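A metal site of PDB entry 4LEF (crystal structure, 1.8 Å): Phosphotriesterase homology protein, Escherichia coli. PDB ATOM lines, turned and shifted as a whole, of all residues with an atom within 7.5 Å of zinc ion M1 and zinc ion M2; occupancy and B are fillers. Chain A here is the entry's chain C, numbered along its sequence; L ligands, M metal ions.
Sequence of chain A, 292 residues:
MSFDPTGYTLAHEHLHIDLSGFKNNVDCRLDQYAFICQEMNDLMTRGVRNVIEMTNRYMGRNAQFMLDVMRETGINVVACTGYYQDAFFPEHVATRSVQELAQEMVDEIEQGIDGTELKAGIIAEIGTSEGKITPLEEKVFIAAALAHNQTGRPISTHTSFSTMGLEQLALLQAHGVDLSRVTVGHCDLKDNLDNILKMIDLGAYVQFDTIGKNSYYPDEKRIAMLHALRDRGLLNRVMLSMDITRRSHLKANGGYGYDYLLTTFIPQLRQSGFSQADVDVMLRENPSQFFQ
The backbone carbonyl oxygen (O) of Met 54 lies close to the backbone NH (N) of Glu 125 (3.5 Å).
A ring nitrogen (ND1) of His 186 sits at hydrogen-bond distance from the side-chain carboxylate of Asp 209 (2.8 Å).
The side-chain hydroxyl (OG1) of Thr 55 is in hydrogen-bond range of a ring nitrogen (ND1) of His 14 (2.8 Å).
NE2 of His 158 sits at hydrogen-bond distance from NE2 of Gln 85.
A ring nitrogen (NE2) of His 158 lies within hydrogen-bond range of the side-chain hydroxyl (OG) of Ser 160 (2.8 Å).
The backbone NH (N) of His 158 lies within hydrogen-bond range of the backbone carbonyl oxygen (O) of Ile 126 (2.8 Å).
OD2 of Asp 243 is in salt-bridge range of NZ of Lys 213 (3.5 Å).
O of Tyr 84 lies within hydrogen-bond range of N of Gly 127.
Within 4 Å of zinc ion M1: His 12, His 14, Glu 125 and Asp 243.
Along chain A the residues within 4 Å of zinc ion M1 span positions 12 to 243.
The nearest printed residue that does not touch zinc ion M1 is Met 54 (4.2 Å).
Tyr 84 touches zinc ion M2 (CE1 to ZN, 3.96 Å).
Of the 25 residues printed, 4 come within 4 Å of zinc ion M2.
The nearest printed residue that does not touch zinc ion M2 is His 12 (4.1 Å).
Zinc ion M1 is bound by O1 of the ligand (1.9 Å), NE2 of His 12 (2.0 Å), OE2 of Glu 125 (2.1 Å), NE2 of His 14 (2.1 Å) and OD1 of Asp 243 (2.5 Å).
Zinc ion M2 is bound by OE1 of Glu 125 (2.0 Å), O3 of the ligand (2.0 Å), NE2 of His 186 (2.0 Å) and ND1 of His 158 (2.1 Å).
Zinc ion M2 has four donor atoms within binding distance.
Slightly farther from zinc ion M2 lies O1 of the ligand (2.8 Å).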
ATOM      1  N   HIS A  12      33.451  10.046 -17.204  1.00  0.00           N
ATOM      2  CA  HIS A  12      32.413  10.462 -16.272  1.00  0.00           C
ATOM      3  C   HIS A  12      31.597  11.585 -16.864  1.00  0.00           C
ATOM      4  O   HIS A  12      32.029  12.738 -16.861  1.00  0.00           O
ATOM      5  CB  HIS A  12      33.028  10.910 -14.923  1.00  0.00           C
ATOM      6  CG  HIS A  12      32.006  11.303 -13.906  1.00  0.00           C
ATOM      7  ND1 HIS A  12      31.947  10.715 -12.652  1.00  0.00           N
ATOM      8  CD2 HIS A  12      31.033  12.241 -13.920  1.00  0.00           C
ATOM      9  CE1 HIS A  12      30.966  11.261 -11.960  1.00  0.00           C
ATOM     10  NE2 HIS A  12      30.397  12.192 -12.707  1.00  0.00           N
ATOM     11  N   GLU A  13      30.421  11.242 -17.379  1.00  0.00           N
ATOM     12  CA  GLU A  13      29.550  12.221 -18.028  1.00  0.00           C
ATOM     13  C   GLU A  13      28.092  11.948 -17.681  1.00  0.00           C
ATOM     14  O   GLU A  13      27.749  10.878 -17.181  1.00  0.00           O
ATOM     15  CB  GLU A  13      29.697  12.158 -19.557  1.00  0.00           C
ATOM     16  CG  GLU A  13      31.078  12.516 -20.067  1.00  0.00           C
ATOM     17  CD  GLU A  13      31.521  13.891 -19.654  1.00  0.00           C
ATOM     18  OE1 GLU A  13      30.639  14.725 -19.367  1.00  0.00           O
ATOM     19  OE2 GLU A  13      32.756  14.124 -19.608  1.00  0.00           O
ATOM     20  N   HIS A  14      27.237  12.934 -17.928  1.00  0.00           N
ATOM     21  CA  HIS A  14      25.800  12.728 -17.827  1.00  0.00           C
ATOM     22  C   HIS A  14      25.213  13.113 -19.177  1.00  0.00           C
ATOM     23  O   HIS A  14      25.670  14.088 -19.780  1.00  0.00           O
ATOM     24  CB  HIS A  14      25.220  13.573 -16.708  1.00  0.00           C
ATOM     25  CG  HIS A  14      25.817  13.241 -15.368  1.00  0.00           C
ATOM     26  ND1 HIS A  14      25.346  12.198 -14.592  1.00  0.00           N
ATOM     27  CD2 HIS A  14      26.882  13.754 -14.712  1.00  0.00           C
ATOM     28  CE1 HIS A  14      26.090  12.104 -13.501  1.00  0.00           C
ATOM     29  NE2 HIS A  14      27.028  13.030 -13.545  1.00  0.00           N
ATOM     30  N   ILE A  17      20.276  13.802 -16.798  1.00  0.00           N
ATOM     31  CA  ILE A  17      20.260  13.794 -15.340  1.00  0.00           C
ATOM     32  C   ILE A  17      19.254  14.841 -14.907  1.00  0.00           C
ATOM     33  O   ILE A  17      19.086  15.844 -15.591  1.00  0.00           O
ATOM     34  CB  ILE A  17      21.659  14.087 -14.775  1.00  0.00           C
ATOM     35  CG1 ILE A  17      21.621  14.248 -13.235  1.00  0.00           C
ATOM     36  CG2 ILE A  17      22.270  15.322 -15.457  1.00  0.00           C
ATOM     37  CD1 ILE A  17      23.004  14.303 -12.606  1.00  0.00           C
ATOM     38  N   GLU A  53      28.217   6.872 -18.648  1.00  0.00           N
ATOM     39  CA  GLU A  53      27.166   7.741 -18.143  1.00  0.00           C
ATOM     40  C   GLU A  53      26.921   7.452 -16.665  1.00  0.00           C
ATOM     41  O   GLU A  53      26.718   6.304 -16.264  1.00  0.00           O
ATOM     42  CB  GLU A  53      25.893   7.547 -18.983  1.00  0.00           C
ATOM     43  CG  GLU A  53      25.082   8.819 -19.190  1.00  0.00           C
ATOM     44  CD  GLU A  53      24.130   9.106 -18.039  1.00  0.00           C
ATOM     45  OE1 GLU A  53      24.034   8.249 -17.128  1.00  0.00           O
ATOM     46  OE2 GLU A  53      23.492  10.173 -18.045  1.00  0.00           O
ATOM     47  N   MET A  54      26.957   8.502 -15.846  1.00  0.00           N
ATOM     48  CA  MET A  54      27.010   8.398 -14.396  1.00  0.00           C
ATOM     49  C   MET A  54      25.690   8.659 -13.664  1.00  0.00           C
ATOM     50  O   MET A  54      25.679   8.806 -12.435  1.00  0.00           O
ATOM     51  CB  MET A  54      28.069   9.381 -13.868  1.00  0.00           C
ATOM     52  CG  MET A  54      29.496   9.143 -14.412  1.00  0.00           C
ATOM     53  SD  MET A  54      30.380   7.821 -13.536  1.00  0.00           S
ATOM     54  CE  MET A  54      30.060   6.414 -14.592  1.00  0.00           C
ATOM     55  N   THR A  55      24.583   8.716 -14.407  1.00  0.00           N
ATOM     56  CA  THR A  55      23.292   9.005 -13.780  1.00  0.00           C
ATOM     57  C   THR A  55      22.610   7.712 -13.353  1.00  0.00           C
ATOM     58  O   THR A  55      22.143   6.964 -14.206  1.00  0.00           O
ATOM     59  CB  THR A  55      22.360   9.746 -14.755  1.00  0.00           C
ATOM     60  OG1 THR A  55      23.077  10.795 -15.413  1.00  0.00           O
ATOM     61  CG2 THR A  55      21.168  10.356 -14.004  1.00  0.00           C
ATOM     62  N   MET A  59      18.854   9.728  -9.665  1.00  0.00           N
ATOM     63  CA  MET A  59      19.403  11.002 -10.139  1.00  0.00           C
ATOM     64  C   MET A  59      18.689  11.447 -11.425  1.00  0.00           C
ATOM     65  O   MET A  59      19.059  12.451 -12.051  1.00  0.00           O
ATOM     66  CB  MET A  59      20.905  10.896 -10.434  1.00  0.00           C
ATOM     67  CG  MET A  59      21.787  10.499  -9.237  1.00  0.00           C
ATOM     68  SD  MET A  59      23.472  10.005  -9.735  1.00  0.00           S
ATOM     69  CE  MET A  59      24.215  11.575 -10.232  1.00  0.00           C
ATOM     70  N   TYR A  84      23.332   7.572  -5.196  1.00  0.00           N
ATOM     71  CA  TYR A  84      24.224   8.715  -5.371  1.00  0.00           C
ATOM     72  C   TYR A  84      24.967   9.136  -4.084  1.00  0.00           C
ATOM     73  O   TYR A  84      26.139   8.792  -3.906  1.00  0.00           O
ATOM     74  CB  TYR A  84      23.416   9.873  -5.990  1.00  0.00           C
ATOM     75  CG  TYR A  84      24.173  11.128  -6.342  1.00  0.00           C
ATOM     76  CD1 TYR A  84      25.520  11.104  -6.694  1.00  0.00           C
ATOM     77  CD2 TYR A  84      23.524  12.365  -6.307  1.00  0.00           C
ATOM     78  CE1 TYR A  84      26.204  12.289  -7.019  1.00  0.00           C
ATOM     79  CE2 TYR A  84      24.186  13.542  -6.616  1.00  0.00           C
ATOM     80  CZ  TYR A  84      25.517  13.500  -6.979  1.00  0.00           C
ATOM     81  OH  TYR A  84      26.136  14.697  -7.263  1.00  0.00           O
ATOM     82  N   GLN A  85      24.312   9.892  -3.213  1.00  0.00           N
ATOM     83  CA  GLN A  85      24.935  10.321  -1.965  1.00  0.00           C
ATOM     84  C   GLN A  85      23.844  10.673  -0.969  1.00  0.00           C
ATOM     85  O   GLN A  85      22.676  10.770  -1.332  1.00  0.00           O
ATOM     86  CB  GLN A  85      25.905  11.496  -2.188  1.00  0.00           C
ATOM     87  CG  GLN A  85      25.301  12.721  -2.889  1.00  0.00           C
ATOM     88  CD  GLN A  85      26.218  13.933  -2.849  1.00  0.00           C
ATOM     89  OE1 GLN A  85      26.584  14.403  -1.765  1.00  0.00           O
ATOM     90  NE2 GLN A  85      26.618  14.439  -4.020  1.00  0.00           N
ATOM     91  N   GLU A 125      27.315   6.672 -10.215  1.00  0.00           N
ATOM     92  CA  GLU A 125      28.454   7.176  -9.460  1.00  0.00           C
ATOM     93  C   GLU A 125      28.043   7.059  -8.010  1.00  0.00           C
ATOM     94  O   GLU A 125      27.057   7.647  -7.599  1.00  0.00           O
ATOM     95  CB  GLU A 125      28.824   8.629  -9.829  1.00  0.00           C
ATOM     96  CG  GLU A 125      27.707   9.677  -9.850  1.00  0.00           C
ATOM     97  CD  GLU A 125      28.279  11.067 -10.066  1.00  0.00           C
ATOM     98  OE1 GLU A 125      29.099  11.493  -9.229  1.00  0.00           O
ATOM     99  OE2 GLU A 125      27.920  11.742 -11.052  1.00  0.00           O
ATOM    100  N   ILE A 126      28.732   6.203  -7.266  1.00  0.00           N
ATOM    101  CA  ILE A 126      28.355   6.012  -5.874  1.00  0.00           C
ATOM    102  C   ILE A 126      29.189   6.919  -5.000  1.00  0.00           C
ATOM    103  O   ILE A 126      30.414   6.910  -5.049  1.00  0.00           O
ATOM    104  CB  ILE A 126      28.420   4.523  -5.468  1.00  0.00           C
ATOM    105  CG1 ILE A 126      29.827   3.988  -5.612  1.00  0.00           C
ATOM    106  CG2 ILE A 126      27.444   3.691  -6.319  1.00  0.00           C
ATOM    107  CD1 ILE A 126      30.053   2.672  -4.877  1.00  0.00           C
ATOM    108  N   GLY A 127      28.514   7.744  -4.206  1.00  0.00           N
ATOM    109  CA  GLY A 127      29.209   8.840  -3.571  1.00  0.00           C
ATOM    110  C   GLY A 127      29.219   8.893  -2.065  1.00  0.00           C
ATOM    111  O   GLY A 127      28.426   8.239  -1.387  1.00  0.00           O
ATOM    112  N   THR A 157      33.271   6.021  -8.387  1.00  0.00           N
ATOM    113  CA  THR A 157      32.748   6.723  -7.216  1.00  0.00           C
ATOM    114  C   THR A 157      32.618   8.229  -7.420  1.00  0.00           C
ATOM    115  O   THR A 157      33.134   8.787  -8.385  1.00  0.00           O
ATOM    116  CB  THR A 157      33.615   6.514  -5.983  1.00  0.00           C
ATOM    117  OG1 THR A 157      34.782   7.348  -6.084  1.00  0.00           O
ATOM    118  CG2 THR A 157      34.034   5.071  -5.856  1.00  0.00           C
ATOM    119  N   HIS A 158      31.902   8.849  -6.503  1.00  0.00           N
ATOM    120  CA  HIS A 158      31.791  10.281  -6.403  1.00  0.00           C
ATOM    121  C   HIS A 158      32.493  10.694  -5.116  1.00  0.00           C
ATOM    122  O   HIS A 158      32.172  10.176  -4.035  1.00  0.00           O
ATOM    123  CB  HIS A 158      30.318  10.695  -6.336  1.00  0.00           C
ATOM    124  CG  HIS A 158      30.088  12.056  -5.762  1.00  0.00           C
ATOM    125  ND1 HIS A 158      29.813  13.158  -6.546  1.00  0.00           N
ATOM    126  CD2 HIS A 158      30.039  12.499  -4.477  1.00  0.00           C
ATOM    127  CE1 HIS A 158      29.656  14.220  -5.779  1.00  0.00           C
ATOM    128  NE2 HIS A 158      29.780  13.851  -4.511  1.00  0.00           N
ATOM    129  N   THR A 159      33.450  11.623  -5.197  1.00  0.00           N
ATOM    130  CA  THR A 159      33.913  12.289  -3.981  1.00  0.00           C
ATOM    131  C   THR A 159      33.396  13.727  -3.922  1.00  0.00           C
ATOM    132  O   THR A 159      33.288  14.408  -4.939  1.00  0.00           O
ATOM    133  CB  THR A 159      35.442  12.253  -3.811  1.00  0.00           C
ATOM    134  OG1 THR A 159      36.064  12.931  -4.902  1.00  0.00           O
ATOM    135  CG2 THR A 159      35.943  10.804  -3.754  1.00  0.00           C
ATOM    136  N   SER A 160      33.013  14.155  -2.727  1.00  0.00           N
ATOM    137  CA  SER A 160      32.537  15.523  -2.541  1.00  0.00           C
ATOM    138  C   SER A 160      33.721  16.401  -2.154  1.00  0.00           C
ATOM    139  O   SER A 160      34.357  16.172  -1.127  1.00  0.00           O
ATOM    140  CB  SER A 160      31.444  15.568  -1.471  1.00  0.00           C
ATOM    141  OG  SER A 160      30.324  14.781  -1.873  1.00  0.00           O
ATOM    142  N   GLY A 185      36.100   9.218  -8.509  1.00  0.00           N
ATOM    143  CA  GLY A 185      35.664  10.419  -9.217  1.00  0.00           C
ATOM    144  C   GLY A 185      35.966  11.729  -8.508  1.00  0.00           C
ATOM    145  O   GLY A 185      36.101  11.773  -7.284  1.00  0.00           O
ATOM    146  N   HIS A 186      36.076  12.793  -9.304  1.00  0.00           N
ATOM    147  CA  HIS A 186      36.224  14.159  -8.807  1.00  0.00           C
ATOM    148  C   HIS A 186      37.483  14.362  -7.963  1.00  0.00           C
ATOM    149  O   HIS A 186      37.449  15.004  -6.905  1.00  0.00           O
ATOM    150  CB  HIS A 186      34.992  14.612  -7.987  1.00  0.00           C
ATOM    151  CG  HIS A 186      33.665  14.261  -8.613  1.00  0.00           C
ATOM    152  ND1 HIS A 186      33.435  14.263  -9.974  1.00  0.00           N
ATOM    153  CD2 HIS A 186      32.478  13.907  -8.033  1.00  0.00           C
ATOM    154  CE1 HIS A 186      32.178  13.927 -10.205  1.00  0.00           C
ATOM    155  NE2 HIS A 186      31.579  13.708  -9.047  1.00  0.00           N
ATOM    156  N   ASP A 209      37.815  14.668 -13.621  1.00  0.00           N
ATOM    157  CA  ASP A 209      36.602  14.656 -14.422  1.00  0.00           C
ATOM    158  C   ASP A 209      35.805  15.943 -14.274  1.00  0.00           C
ATOM    159  O   ASP A 209      34.639  16.004 -14.649  1.00  0.00           O
ATOM    160  CB  ASP A 209      35.750  13.419 -14.093  1.00  0.00           C
ATOM    161  CG  ASP A 209      35.529  13.267 -12.598  1.00  0.00           C
ATOM    162  OD1 ASP A 209      35.493  14.314 -11.919  1.00  0.00           O
ATOM    163  OD2 ASP A 209      35.403  12.115 -12.119  1.00  0.00           O
ATOM    164  N   THR A 210      36.421  17.001 -13.751  1.00  0.00           N
ATOM    165  CA  THR A 210      35.719  18.281 -13.679  1.00  0.00           C
ATOM    166  C   THR A 210      36.448  19.360 -14.459  1.00  0.00           C
ATOM    167  O   THR A 210      36.421  20.538 -14.088  1.00  0.00           O
ATOM    168  CB  THR A 210      35.438  18.730 -12.231  1.00  0.00           C
ATOM    169  OG1 THR A 210      36.671  18.927 -11.532  1.00  0.00           O
ATOM    170  CG2 THR A 210      34.590  17.686 -11.475  1.00  0.00           C
ATOM    171  N   LYS A 213      35.388  23.141 -15.022  1.00  0.00           N
ATOM    172  CA  LYS A 213      34.663  23.694 -13.866  1.00  0.00           C
ATOM    173  C   LYS A 213      35.607  24.578 -13.070  1.00  0.00           C
ATOM    174  O   LYS A 213      36.054  24.204 -11.981  1.00  0.00           O
ATOM    175  CB  LYS A 213      34.037  22.596 -13.006  1.00  0.00           C
ATOM    176  CG  LYS A 213      33.215  21.622 -13.861  1.00  0.00           C
ATOM    177  CD  LYS A 213      32.203  20.812 -13.073  1.00  0.00           C
ATOM    178  CE  LYS A 213      31.335  20.006 -14.047  1.00  0.00           C
ATOM    179  NZ  LYS A 213      30.086  19.457 -13.439  1.00  0.00           N
ATOM    180  N   ASP A 243      32.375  15.887 -16.943  1.00  0.00           N
ATOM    181  CA  ASP A 243      31.233  15.765 -16.009  1.00  0.00           C
ATOM    182  C   ASP A 243      30.172  16.822 -16.316  1.00  0.00           C
ATOM    183  O   ASP A 243      29.760  17.574 -15.434  1.00  0.00           O
ATOM    184  CB  ASP A 243      31.688  15.849 -14.535  1.00  0.00           C
ATOM    185  CG  ASP A 243      30.557  15.595 -13.554  1.00  0.00           C
ATOM    186  OD1 ASP A 243      29.627  14.825 -13.879  1.00  0.00           O
ATOM    187  OD2 ASP A 243      30.599  16.191 -12.450  1.00  0.00           O
ATOM    188  N   ILE A 244      29.739  16.885 -17.561  1.00  0.00           N
ATOM    189  CA  ILE A 244      28.618  17.761 -17.906  1.00  0.00           C
ATOM    190  C   ILE A 244      27.378  17.393 -17.093  1.00  0.00           C
ATOM    191  O   ILE A 244      26.964  16.238 -17.078  1.00  0.00           O
ATOM    192  CB  ILE A 244      28.270  17.633 -19.380  1.00  0.00           C
ATOM    193  CG1 ILE A 244      29.488  17.963 -20.234  1.00  0.00           C
ATOM    194  CG2 ILE A 244      27.050  18.472 -19.715  1.00  0.00           C
ATOM    195  CD1 ILE A 244      30.036  19.394 -20.049  1.00  0.00           C
ATOM    196  N   THR A 245      26.797  18.363 -16.402  1.00  0.00           N
ATOM    197  CA  THR A 245      25.670  18.086 -15.501  1.00  0.00           C
ATOM    198  C   THR A 245      24.544  19.074 -15.681  1.00  0.00           C
ATOM    199  O   THR A 245      23.460  18.872 -15.118  1.00  0.00           O
ATOM    200  CB  THR A 245      26.096  18.198 -14.021  1.00  0.00           C
ATOM    201  OG1 THR A 245      26.730  19.458 -13.789  1.00  0.00           O
ATOM    202  CG2 THR A 245      27.019  17.057 -13.628  1.00  0.00           C
HETATM  203  P1  LIG L   1      28.084  15.286 -10.029  1.00  0.00           P
HETATM  204  O1  LIG L   1      28.982  14.604 -11.015  1.00  0.00           O
HETATM  205  O2  LIG L   1      26.620  15.278 -10.415  1.00  0.00           O
HETATM  206  O3  LIG L   1      28.207  14.568  -8.687  1.00  0.00           O
HETATM  207  O4  LIG L   1      28.573  16.693  -9.921  1.00  0.00           O
HETATM  208 ZN    ZN M   1      28.658  13.188 -12.306  1.00  0.00          ZN
HETATM  209 ZN    ZN M   2      29.681  13.267  -8.634  1.00  0.00          ZN
